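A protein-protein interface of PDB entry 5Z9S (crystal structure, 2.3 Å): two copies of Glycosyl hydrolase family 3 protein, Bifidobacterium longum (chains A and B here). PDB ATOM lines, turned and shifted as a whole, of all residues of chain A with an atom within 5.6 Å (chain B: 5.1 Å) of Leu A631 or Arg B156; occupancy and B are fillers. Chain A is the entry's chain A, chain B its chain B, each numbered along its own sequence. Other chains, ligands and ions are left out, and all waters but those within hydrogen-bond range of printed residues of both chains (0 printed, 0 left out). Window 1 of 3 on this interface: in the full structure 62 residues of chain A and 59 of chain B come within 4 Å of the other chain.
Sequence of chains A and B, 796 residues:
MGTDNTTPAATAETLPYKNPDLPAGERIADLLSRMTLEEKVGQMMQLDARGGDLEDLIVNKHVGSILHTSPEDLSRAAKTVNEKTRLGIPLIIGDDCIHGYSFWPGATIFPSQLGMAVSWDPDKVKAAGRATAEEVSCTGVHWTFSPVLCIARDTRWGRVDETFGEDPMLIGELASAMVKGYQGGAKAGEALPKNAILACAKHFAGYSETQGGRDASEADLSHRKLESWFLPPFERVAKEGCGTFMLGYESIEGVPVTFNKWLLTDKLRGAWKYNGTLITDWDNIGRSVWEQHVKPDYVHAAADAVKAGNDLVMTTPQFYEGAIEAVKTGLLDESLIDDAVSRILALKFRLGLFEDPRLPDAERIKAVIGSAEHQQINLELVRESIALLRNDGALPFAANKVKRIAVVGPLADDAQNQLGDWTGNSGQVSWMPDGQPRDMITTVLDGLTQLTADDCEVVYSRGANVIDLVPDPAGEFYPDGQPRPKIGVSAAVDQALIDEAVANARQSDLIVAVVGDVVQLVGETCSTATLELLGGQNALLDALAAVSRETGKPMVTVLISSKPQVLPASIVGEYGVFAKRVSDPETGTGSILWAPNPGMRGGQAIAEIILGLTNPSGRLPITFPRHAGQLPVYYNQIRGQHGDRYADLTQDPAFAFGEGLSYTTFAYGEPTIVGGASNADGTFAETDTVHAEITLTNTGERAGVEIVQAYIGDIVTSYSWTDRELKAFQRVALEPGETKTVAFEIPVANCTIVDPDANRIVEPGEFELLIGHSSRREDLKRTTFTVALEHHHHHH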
ATOM      1  N   ASP A 154     -23.553 -28.473   8.202  1.00  0.00           N
ATOM      2  CA  ASP A 154     -23.748 -27.046   7.944  1.00  0.00           C
ATOM      3  C   ASP A 154     -23.750 -26.327   9.286  1.00  0.00           C
ATOM      4  O   ASP A 154     -24.674 -26.512  10.086  1.00  0.00           O
ATOM      5  CB  ASP A 154     -25.052 -26.797   7.182  1.00  0.00           C
ATOM      6  CG  ASP A 154     -25.133 -25.399   6.579  1.00  0.00           C
ATOM      7  OD1 ASP A 154     -25.598 -25.283   5.424  1.00  0.00           O
ATOM      8  OD2 ASP A 154     -24.739 -24.419   7.244  1.00  0.00           O
ATOM      9  N   THR A 155     -22.730 -25.499   9.526  1.00  0.00           N
ATOM     10  CA  THR A 155     -22.585 -24.841  10.819  1.00  0.00           C
ATOM     11  C   THR A 155     -23.739 -23.899  11.124  1.00  0.00           C
ATOM     12  O   THR A 155     -23.986 -23.598  12.297  1.00  0.00           O
ATOM     13  CB  THR A 155     -21.276 -24.049  10.865  1.00  0.00           C
ATOM     14  OG1 THR A 155     -20.269 -24.737  10.116  1.00  0.00           O
ATOM     15  CG2 THR A 155     -20.802 -23.877  12.304  1.00  0.00           C
ATOM     16  N   ARG A 156     -24.458 -23.439  10.099  1.00  0.00           N
ATOM     17  CA  ARG A 156     -25.603 -22.567  10.312  1.00  0.00           C
ATOM     18  C   ARG A 156     -26.754 -23.272  11.016  1.00  0.00           C
ATOM     19  O   ARG A 156     -27.570 -22.603  11.658  1.00  0.00           O
ATOM     20  CB  ARG A 156     -26.073 -22.001   8.973  1.00  0.00           C
ATOM     21  CG  ARG A 156     -25.097 -21.021   8.353  1.00  0.00           C
ATOM     22  CD  ARG A 156     -25.580 -20.551   6.998  1.00  0.00           C
ATOM     23  NE  ARG A 156     -25.626 -21.648   6.038  1.00  0.00           N
ATOM     24  CZ  ARG A 156     -26.042 -21.528   4.783  1.00  0.00           C
ATOM     25  NH1 ARG A 156     -26.451 -20.351   4.327  1.00  0.00           N
ATOM     26  NH2 ARG A 156     -26.048 -22.584   3.984  1.00  0.00           N
ATOM     27  N   LEU A 531     -22.876 -16.759  12.115  1.00  0.00           N
ATOM     28  CA  LEU A 531     -22.043 -17.561  13.009  1.00  0.00           C
ATOM     29  C   LEU A 531     -21.180 -16.709  13.936  1.00  0.00           C
ATOM     30  O   LEU A 531     -20.308 -17.244  14.629  1.00  0.00           O
ATOM     31  CB  LEU A 531     -21.152 -18.535  12.227  1.00  0.00           C
ATOM     32  CG  LEU A 531     -21.839 -19.403  11.173  1.00  0.00           C
ATOM     33  CD1 LEU A 531     -20.817 -20.237  10.431  1.00  0.00           C
ATOM     34  CD2 LEU A 531     -22.898 -20.284  11.807  1.00  0.00           C
ATOM     35  N   PRO A 625     -15.488 -22.809  10.683  1.00  0.00           N
ATOM     36  CA  PRO A 625     -15.300 -21.948   9.514  1.00  0.00           C
ATOM     37  C   PRO A 625     -14.818 -20.562   9.911  1.00  0.00           C
ATOM     38  O   PRO A 625     -15.063 -20.083  11.020  1.00  0.00           O
ATOM     39  CB  PRO A 625     -16.701 -21.886   8.897  1.00  0.00           C
ATOM     40  CG  PRO A 625     -17.616 -22.065  10.059  1.00  0.00           C
ATOM     41  CD  PRO A 625     -16.912 -23.007  11.002  1.00  0.00           C
ATOM     42  N   HIS A 627     -15.757 -17.969   7.989  1.00  0.00           N
ATOM     43  CA  HIS A 627     -16.855 -17.126   7.542  1.00  0.00           C
ATOM     44  C   HIS A 627     -17.967 -18.035   7.043  1.00  0.00           C
ATOM     45  O   HIS A 627     -17.713 -19.160   6.603  1.00  0.00           O
ATOM     46  CB  HIS A 627     -16.395 -16.160   6.443  1.00  0.00           C
ATOM     47  CG  HIS A 627     -17.379 -15.075   6.130  1.00  0.00           C
ATOM     48  ND1 HIS A 627     -18.433 -15.253   5.258  1.00  0.00           N
ATOM     49  CD2 HIS A 627     -17.464 -13.797   6.566  1.00  0.00           C
ATOM     50  CE1 HIS A 627     -19.126 -14.131   5.176  1.00  0.00           C
ATOM     51  NE2 HIS A 627     -18.560 -13.233   5.960  1.00  0.00           N
ATOM     52  N   ALA A 628     -19.205 -17.543   7.126  1.00  0.00           N
ATOM     53  CA  ALA A 628     -20.339 -18.329   6.654  1.00  0.00           C
ATOM     54  C   ALA A 628     -20.228 -18.639   5.167  1.00  0.00           C
ATOM     55  O   ALA A 628     -20.675 -19.702   4.720  1.00  0.00           O
ATOM     56  CB  ALA A 628     -21.645 -17.595   6.944  1.00  0.00           C
ATOM     57  N   GLY A 629     -19.632 -17.735   4.389  1.00  0.00           N
ATOM     58  CA  GLY A 629     -19.414 -17.967   2.972  1.00  0.00           C
ATOM     59  C   GLY A 629     -18.405 -19.051   2.663  1.00  0.00           C
ATOM     60  O   GLY A 629     -18.268 -19.432   1.495  1.00  0.00           O
ATOM     61  N   GLN A 630     -17.696 -19.549   3.677  1.00  0.00           N
ATOM     62  CA  GLN A 630     -16.768 -20.655   3.493  1.00  0.00           C
ATOM     63  C   GLN A 630     -17.475 -22.003   3.406  1.00  0.00           C
ATOM     64  O   GLN A 630     -16.869 -22.975   2.944  1.00  0.00           O
ATOM     65  CB  GLN A 630     -15.765 -20.677   4.648  1.00  0.00           C
ATOM     66  CG  GLN A 630     -14.342 -21.015   4.261  1.00  0.00           C
ATOM     67  CD  GLN A 630     -13.401 -20.968   5.450  1.00  0.00           C
ATOM     68  OE1 GLN A 630     -13.818 -21.166   6.593  1.00  0.00           O
ATOM     69  NE2 GLN A 630     -12.127 -20.685   5.191  1.00  0.00           N
ATOM     70  N   LEU A 631     -18.737 -22.078   3.815  1.00  0.00           N
ATOM     71  CA  LEU A 631     -19.453 -23.349   3.912  1.00  0.00           C
ATOM     72  C   LEU A 631     -19.688 -24.019   2.557  1.00  0.00           C
ATOM     73  O   LEU A 631     -19.919 -23.344   1.556  1.00  0.00           O
ATOM     74  CB  LEU A 631     -20.794 -23.137   4.622  1.00  0.00           C
ATOM     75  CG  LEU A 631     -20.704 -22.636   6.064  1.00  0.00           C
ATOM     76  CD1 LEU A 631     -22.082 -22.498   6.669  1.00  0.00           C
ATOM     77  CD2 LEU A 631     -19.852 -23.581   6.897  1.00  0.00           C
ATOM     78  N   PRO A 632     -19.644 -25.362   2.527  1.00  0.00           N
ATOM     79  CA  PRO A 632     -19.383 -26.255   3.663  1.00  0.00           C
ATOM     80  C   PRO A 632     -17.894 -26.431   3.970  1.00  0.00           C
ATOM     81  O   PRO A 632     -17.069 -26.346   3.059  1.00  0.00           O
ATOM     82  CB  PRO A 632     -19.999 -27.574   3.202  1.00  0.00           C
ATOM     83  CG  PRO A 632     -19.826 -27.555   1.728  1.00  0.00           C
ATOM     84  CD  PRO A 632     -19.984 -26.117   1.306  1.00  0.00           C
ATOM     85  N   VAL A 633     -17.560 -26.687   5.237  1.00  0.00           N
ATOM     86  CA  VAL A 633     -16.177 -26.743   5.685  1.00  0.00           C
ATOM     87  C   VAL A 633     -15.805 -28.096   6.283  1.00  0.00           C
ATOM     88  O   VAL A 633     -14.713 -28.238   6.833  1.00  0.00           O
ATOM     89  CB  VAL A 633     -15.865 -25.611   6.685  1.00  0.00           C
ATOM     90  CG1 VAL A 633     -16.045 -24.254   6.028  1.00  0.00           C
ATOM     91  CG2 VAL A 633     -16.743 -25.736   7.923  1.00  0.00           C
ATOM     92  N   TYR A 646     -11.269 -19.051  -2.547  1.00  0.00           N
ATOM     93  CA  TYR A 646     -12.140 -17.973  -2.980  1.00  0.00           C
ATOM     94  C   TYR A 646     -11.280 -16.750  -3.272  1.00  0.00           C
ATOM     95  O   TYR A 646     -10.204 -16.575  -2.695  1.00  0.00           O
ATOM     96  CB  TYR A 646     -13.183 -17.629  -1.913  1.00  0.00           C
ATOM     97  CG  TYR A 646     -14.186 -18.724  -1.614  1.00  0.00           C
ATOM     98  CD1 TYR A 646     -13.957 -19.642  -0.598  1.00  0.00           C
ATOM     99  CD2 TYR A 646     -15.368 -18.826  -2.334  1.00  0.00           C
ATOM    100  CE1 TYR A 646     -14.868 -20.638  -0.313  1.00  0.00           C
ATOM    101  CE2 TYR A 646     -16.287 -19.818  -2.057  1.00  0.00           C
ATOM    102  CZ  TYR A 646     -16.031 -20.723  -1.045  1.00  0.00           C
ATOM    103  OH  TYR A 646     -16.942 -21.716  -0.762  1.00  0.00           O
ATOM    104  N   ASP B 154     -26.311 -19.734  -6.632  1.00  0.00           N
ATOM    105  CA  ASP B 154     -25.427 -19.404  -5.517  1.00  0.00           C
ATOM    106  C   ASP B 154     -24.626 -18.180  -5.935  1.00  0.00           C
ATOM    107  O   ASP B 154     -23.778 -18.275  -6.827  1.00  0.00           O
ATOM    108  CB  ASP B 154     -24.501 -20.579  -5.191  1.00  0.00           C
ATOM    109  CG  ASP B 154     -23.828 -20.450  -3.837  1.00  0.00           C
ATOM    110  OD1 ASP B 154     -23.701 -21.477  -3.142  1.00  0.00           O
ATOM    111  OD2 ASP B 154     -23.407 -19.336  -3.470  1.00  0.00           O
ATOM    112  N   THR B 155     -24.883 -17.034  -5.300  1.00  0.00           N
ATOM    113  CA  THR B 155     -24.198 -15.814  -5.709  1.00  0.00           C
ATOM    114  C   THR B 155     -22.696 -15.885  -5.464  1.00  0.00           C
ATOM    115  O   THR B 155     -21.952 -15.090  -6.044  1.00  0.00           O
ATOM    116  CB  THR B 155     -24.805 -14.587  -5.022  1.00  0.00           C
ATOM    117  OG1 THR B 155     -23.785 -13.613  -4.774  1.00  0.00           O
ATOM    118  CG2 THR B 155     -25.467 -14.968  -3.735  1.00  0.00           C
ATOM    119  N   ARG B 156     -22.233 -16.817  -4.626  1.00  0.00           N
ATOM    120  CA  ARG B 156     -20.798 -16.978  -4.418  1.00  0.00           C
ATOM    121  C   ARG B 156     -20.083 -17.440  -5.681  1.00  0.00           C
ATOM    122  O   ARG B 156     -18.880 -17.200  -5.821  1.00  0.00           O
ATOM    123  CB  ARG B 156     -20.531 -17.984  -3.293  1.00  0.00           C
ATOM    124  CG  ARG B 156     -20.921 -17.511  -1.909  1.00  0.00           C
ATOM    125  CD  ARG B 156     -20.680 -18.597  -0.875  1.00  0.00           C
ATOM    126  NE  ARG B 156     -21.534 -19.756  -1.102  1.00  0.00           N
ATOM    127  CZ  ARG B 156     -21.511 -20.864  -0.368  1.00  0.00           C
ATOM    128  NH1 ARG B 156     -20.672 -20.972   0.656  1.00  0.00           N
ATOM    129  NH2 ARG B 156     -22.331 -21.865  -0.655  1.00  0.00           N
ATOM    130  N   TRP B 157     -20.798 -18.088  -6.596  1.00  0.00           N
ATOM    131  CA  TRP B 157     -20.193 -18.630  -7.804  1.00  0.00           C
ATOM    132  C   TRP B 157     -19.542 -17.523  -8.626  1.00  0.00           C
ATOM    133  O   TRP B 157     -20.098 -16.433  -8.782  1.00  0.00           O
ATOM    134  CB  TRP B 157     -21.258 -19.354  -8.626  1.00  0.00           C
ATOM    135  CG  TRP B 157     -20.736 -20.322  -9.634  1.00  0.00           C
ATOM    136  CD1 TRP B 157     -19.786 -21.280  -9.437  1.00  0.00           C
ATOM    137  CD2 TRP B 157     -21.169 -20.460 -10.991  1.00  0.00           C
ATOM    138  NE1 TRP B 157     -19.587 -21.992 -10.591  1.00  0.00           N
ATOM    139  CE2 TRP B 157     -20.426 -21.509 -11.560  1.00  0.00           C
ATOM    140  CE3 TRP B 157     -22.109 -19.790 -11.781  1.00  0.00           C
ATOM    141  CZ2 TRP B 157     -20.591 -21.905 -12.883  1.00  0.00           C
ATOM    142  CZ3 TRP B 157     -22.271 -20.183 -13.093  1.00  0.00           C
ATOM    143  CH2 TRP B 157     -21.518 -21.232 -13.632  1.00  0.00           C
ATOM    144  N   GLY B 158     -18.344 -17.803  -9.140  1.00  0.00           N
ATOM    145  CA  GLY B 158     -17.588 -16.782  -9.845  1.00  0.00           C
ATOM    146  C   GLY B 158     -18.135 -16.434 -11.213  1.00  0.00           C
ATOM    147  O   GLY B 158     -17.825 -15.360 -11.737  1.00  0.00           O
ATOM    148  N   GLY B 212     -20.454 -25.161  -2.035  1.00  0.00           N
ATOM    149  CA  GLY B 212     -19.823 -23.916  -1.651  1.00  0.00           C
ATOM    150  C   GLY B 212     -19.802 -22.847  -2.717  1.00  0.00           C
ATOM    151  O   GLY B 212     -19.152 -21.816  -2.523  1.00  0.00           O
ATOM    152  N   GLY B 213     -20.511 -23.044  -3.827  1.00  0.00           N
ATOM    153  CA  GLY B 213     -20.414 -22.116  -4.936  1.00  0.00           C
ATOM    154  C   GLY B 213     -19.050 -22.067  -5.582  1.00  0.00           C
ATOM    155  O   GLY B 213     -18.749 -21.115  -6.304  1.00  0.00           O
ATOM    156  N   ARG B 214     -18.210 -23.066  -5.328  1.00  0.00           N
ATOM    157  CA  ARG B 214     -16.863 -23.102  -5.869  1.00  0.00           C
ATOM    158  C   ARG B 214     -16.876 -23.591  -7.317  1.00  0.00           C
ATOM    159  O   ARG B 214     -17.854 -24.169  -7.798  1.00  0.00           O
ATOM    160  CB  ARG B 214     -15.985 -24.012  -5.011  1.00  0.00           C
ATOM    161  CG  ARG B 214     -15.822 -23.529  -3.577  1.00  0.00           C
ATOM    162  CD  ARG B 214     -15.566 -24.683  -2.620  1.00  0.00           C
ATOM    163  NE  ARG B 214     -16.028 -24.376  -1.269  1.00  0.00           N
ATOM    164  CZ  ARG B 214     -16.177 -25.276  -0.303  1.00  0.00           C
ATOM    165  NH1 ARG B 214     -15.897 -26.551  -0.527  1.00  0.00           N
ATOM    166  NH2 ARG B 214     -16.608 -24.900   0.889  1.00  0.00           N
ATOM    167  N   SER B 527     -14.464 -17.762  -7.432  1.00  0.00           N
ATOM    168  CA  SER B 527     -15.634 -17.559  -6.595  1.00  0.00           C
ATOM    169  C   SER B 527     -15.265 -16.694  -5.391  1.00  0.00           C
ATOM    170  O   SER B 527     -14.102 -16.598  -4.998  1.00  0.00           O
ATOM    171  CB  SER B 527     -16.197 -18.899  -6.125  1.00  0.00           C
ATOM    172  OG  SER B 527     -16.545 -19.719  -7.222  1.00  0.00           O
ATOM    173  N   THR B 528     -16.269 -16.047  -4.810  1.00  0.00           N
ATOM    174  CA  THR B 528     -16.071 -15.241  -3.615  1.00  0.00           C
ATOM    175  C   THR B 528     -16.997 -15.726  -2.511  1.00  0.00           C
ATOM    176  O   THR B 528     -18.125 -16.148  -2.770  1.00  0.00           O
ATOM    177  CB  THR B 528     -16.323 -13.751  -3.872  1.00  0.00           C
ATOM    178  OG1 THR B 528     -17.673 -13.566  -4.311  1.00  0.00           O
ATOM    179  CG2 THR B 528     -15.362 -13.215  -4.925  1.00  0.00           C
ATOM    180  N   ALA B 529     -16.513 -15.654  -1.277  1.00  0.00           N
ATOM    181  CA  ALA B 529     -17.255 -16.157  -0.131  1.00  0.00           C
ATOM    182  C   ALA B 529     -18.026 -15.076   0.614  1.00  0.00           C
ATOM    183  O   ALA B 529     -19.134 -15.337   1.089  1.00  0.00           O
ATOM    184  CB  ALA B 529     -16.308 -16.869   0.838  1.00  0.00           C
ATOM    185  N   LEU B 531     -18.923 -11.861  -0.548  1.00  0.00           N
ATOM    186  CA  LEU B 531     -19.751 -11.036  -1.425  1.00  0.00           C
ATOM    187  C   LEU B 531     -19.612  -9.545  -1.137  1.00  0.00           C
ATOM    188  O   LEU B 531     -20.388  -8.741  -1.665  1.00  0.00           O
ATOM    189  CB  LEU B 531     -21.230 -11.443  -1.352  1.00  0.00           C
ATOM    190  CG  LEU B 531     -21.540 -12.930  -1.523  1.00  0.00           C
ATOM    191  CD1 LEU B 531     -23.029 -13.191  -1.340  1.00  0.00           C
ATOM    192  CD2 LEU B 531     -21.064 -13.432  -2.877  1.00  0.00           C
ATOM    193  N   LYS B 563     -21.668  -9.293 -10.269  1.00  0.00           N
ATOM    194  CA  LYS B 563     -22.739 -10.039  -9.624  1.00  0.00           C
ATOM    195  C   LYS B 563     -23.225  -9.231  -8.428  1.00  0.00           C
ATOM    196  O   LYS B 563     -22.602  -8.227  -8.056  1.00  0.00           O
ATOM    197  CB  LYS B 563     -22.257 -11.436  -9.198  1.00  0.00           C
ATOM    198  CG  LYS B 563     -21.089 -11.423  -8.234  1.00  0.00           C
ATOM    199  CD  LYS B 563     -20.672 -12.832  -7.878  1.00  0.00           C
ATOM    200  CE  LYS B 563     -19.531 -12.832  -6.881  1.00  0.00           C
ATOM    201  NZ  LYS B 563     -19.199 -14.209  -6.441  1.00  0.00           N
ATOM    202  N   ALA B 628     -23.689 -13.699   3.046  1.00  0.00           N
ATOM    203  CA  ALA B 628     -23.463 -15.009   2.445  1.00  0.00           C
ATOM    204  C   ALA B 628     -24.143 -16.121   3.234  1.00  0.00           C
ATOM    205  O   ALA B 628     -24.574 -17.120   2.649  1.00  0.00           O
ATOM    206  CB  ALA B 628     -21.966 -15.282   2.330  1.00  0.00           C
ATOM    207  N   LEU B 631     -27.660 -17.600   2.172  1.00  0.00           N
ATOM    208  CA  LEU B 631     -27.837 -18.423   0.976  1.00  0.00           C
ATOM    209  C   LEU B 631     -28.453 -19.789   1.271  1.00  0.00           C
ATOM    210  O   LEU B 631     -28.201 -20.370   2.322  1.00  0.00           O
ATOM    211  CB  LEU B 631     -26.494 -18.596   0.265  1.00  0.00           C
ATOM    212  CG  LEU B 631     -25.899 -17.268  -0.203  1.00  0.00           C
ATOM    213  CD1 LEU B 631     -24.589 -17.465  -0.956  1.00  0.00           C
ATOM    214  CD2 LEU B 631     -26.918 -16.528  -1.043  1.00  0.00           C
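Along chain B the printed residues that touch a printed residue of chain A span positions 156 to 631. Of the 13 printed residues of chain A, 6 touch a printed residue of chain B. Printed residues of chain A that touch a printed residue of chain B: Arg A156, Gly A629, Gln A630, Leu A631, Pro A632 and Tyr A646. Hydrophobic or aromatic side chains of chain A within 4 Å of the printed part of chain B: Pro A632 and Tyr A646.
O of Leu B631 sits at hydrogen-bond distance from NH1 of Arg A156 (2.7 Å). NH1 of Arg B156 lies within hydrogen-bond range of O of Gly A629, at 3.0 Å. O of Gln A630 is in hydrogen-bond range of NH2 of Arg B214 (2.8 Å). The backbone carbonyl oxygen (O) of Leu A631 is in hydrogen-bond range of the guanidinium group (NH1) of Arg B156, 2.6 Å away. The backbone carbonyl oxygen (O) of Pro A632 lies within hydrogen-bond range of the guanidinium group (NH2) of Arg B214 (2.6 Å). The side-chain hydroxyl of Tyr A646 sits at hydrogen-bond distance from the backbone carbonyl oxygen of Gly B212 (2.8 Å). OH of Tyr A646 sits at hydrogen-bond distance from NE of Arg B214.
The guanidinium group (NH2) of Arg B156 lies within salt-bridge range of the side-chain carboxylate (OD1) of Asp B154 (2.9 Å). NE of Arg B156 sits close to O of Gly B212 (3.5 Å). NZ of Lys B563 is in hydrogen-bond range of O of Arg B156. The side-chain hydroxyl of Ser B527 lies within hydrogen-bond range of the backbone NH of Gly B158, 3.3 Å away. The backbone carbonyl oxygen of Gly B213 is in hydrogen-bond range of the side-chain hydroxyl of Ser B527, 2.8 Å away. The side-chain hydroxyl (OG1) of Thr B528 is in hydrogen-bond range of the side-chain amino group (NZ) of Lys B563 (2.7 Å).
Among the printed residues, pairs that only touch across the chains: Tyr A646 with Ser B527, Gly A629 with Ala B529, Leu A631 with Gly B212, Tyr A646 with Thr B528, Pro A632 with Gly B212, Tyr A646 with Ala B529, Leu A631 with Arg B214 and Gly A629 with Ala B628.
Arg A156 touches Leu B631, and with the chains exchanged Leu A631 touches Arg B156.
Printed residues of chain B within 4 Å of Leu A631: Arg B156 (2.6 Å), Gly B212 (3.3 Å) and Arg B214 (3.6 Å). Of chain A, only Gly A629 and Leu A631 come within 4 Å of Arg B156. Of the printed residues of chain A, Thr B528 touches Tyr A646 (3.5 Å). Printed residues of chain B within 4 Å of Arg A156: Leu B631 (2.7 Å). Of the printed residues of chain B, Tyr A646 touches Gly B212 (2.8 Å), Arg B214 (2.9 Å), Ser B527 (3.1 Å), Thr B528 (3.5 Å) and Ala B529 (3.5 Å). Of the printed residues of chain B, Gln A630 touches Arg B214 (2.8 Å). Trp B157 touches none of the printed residues of chain A. His A627 touches none of the printed residues of chain B. The nearest printed residue of chain B that does not touch Leu A631 is Gly B213 (5.4 Å).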
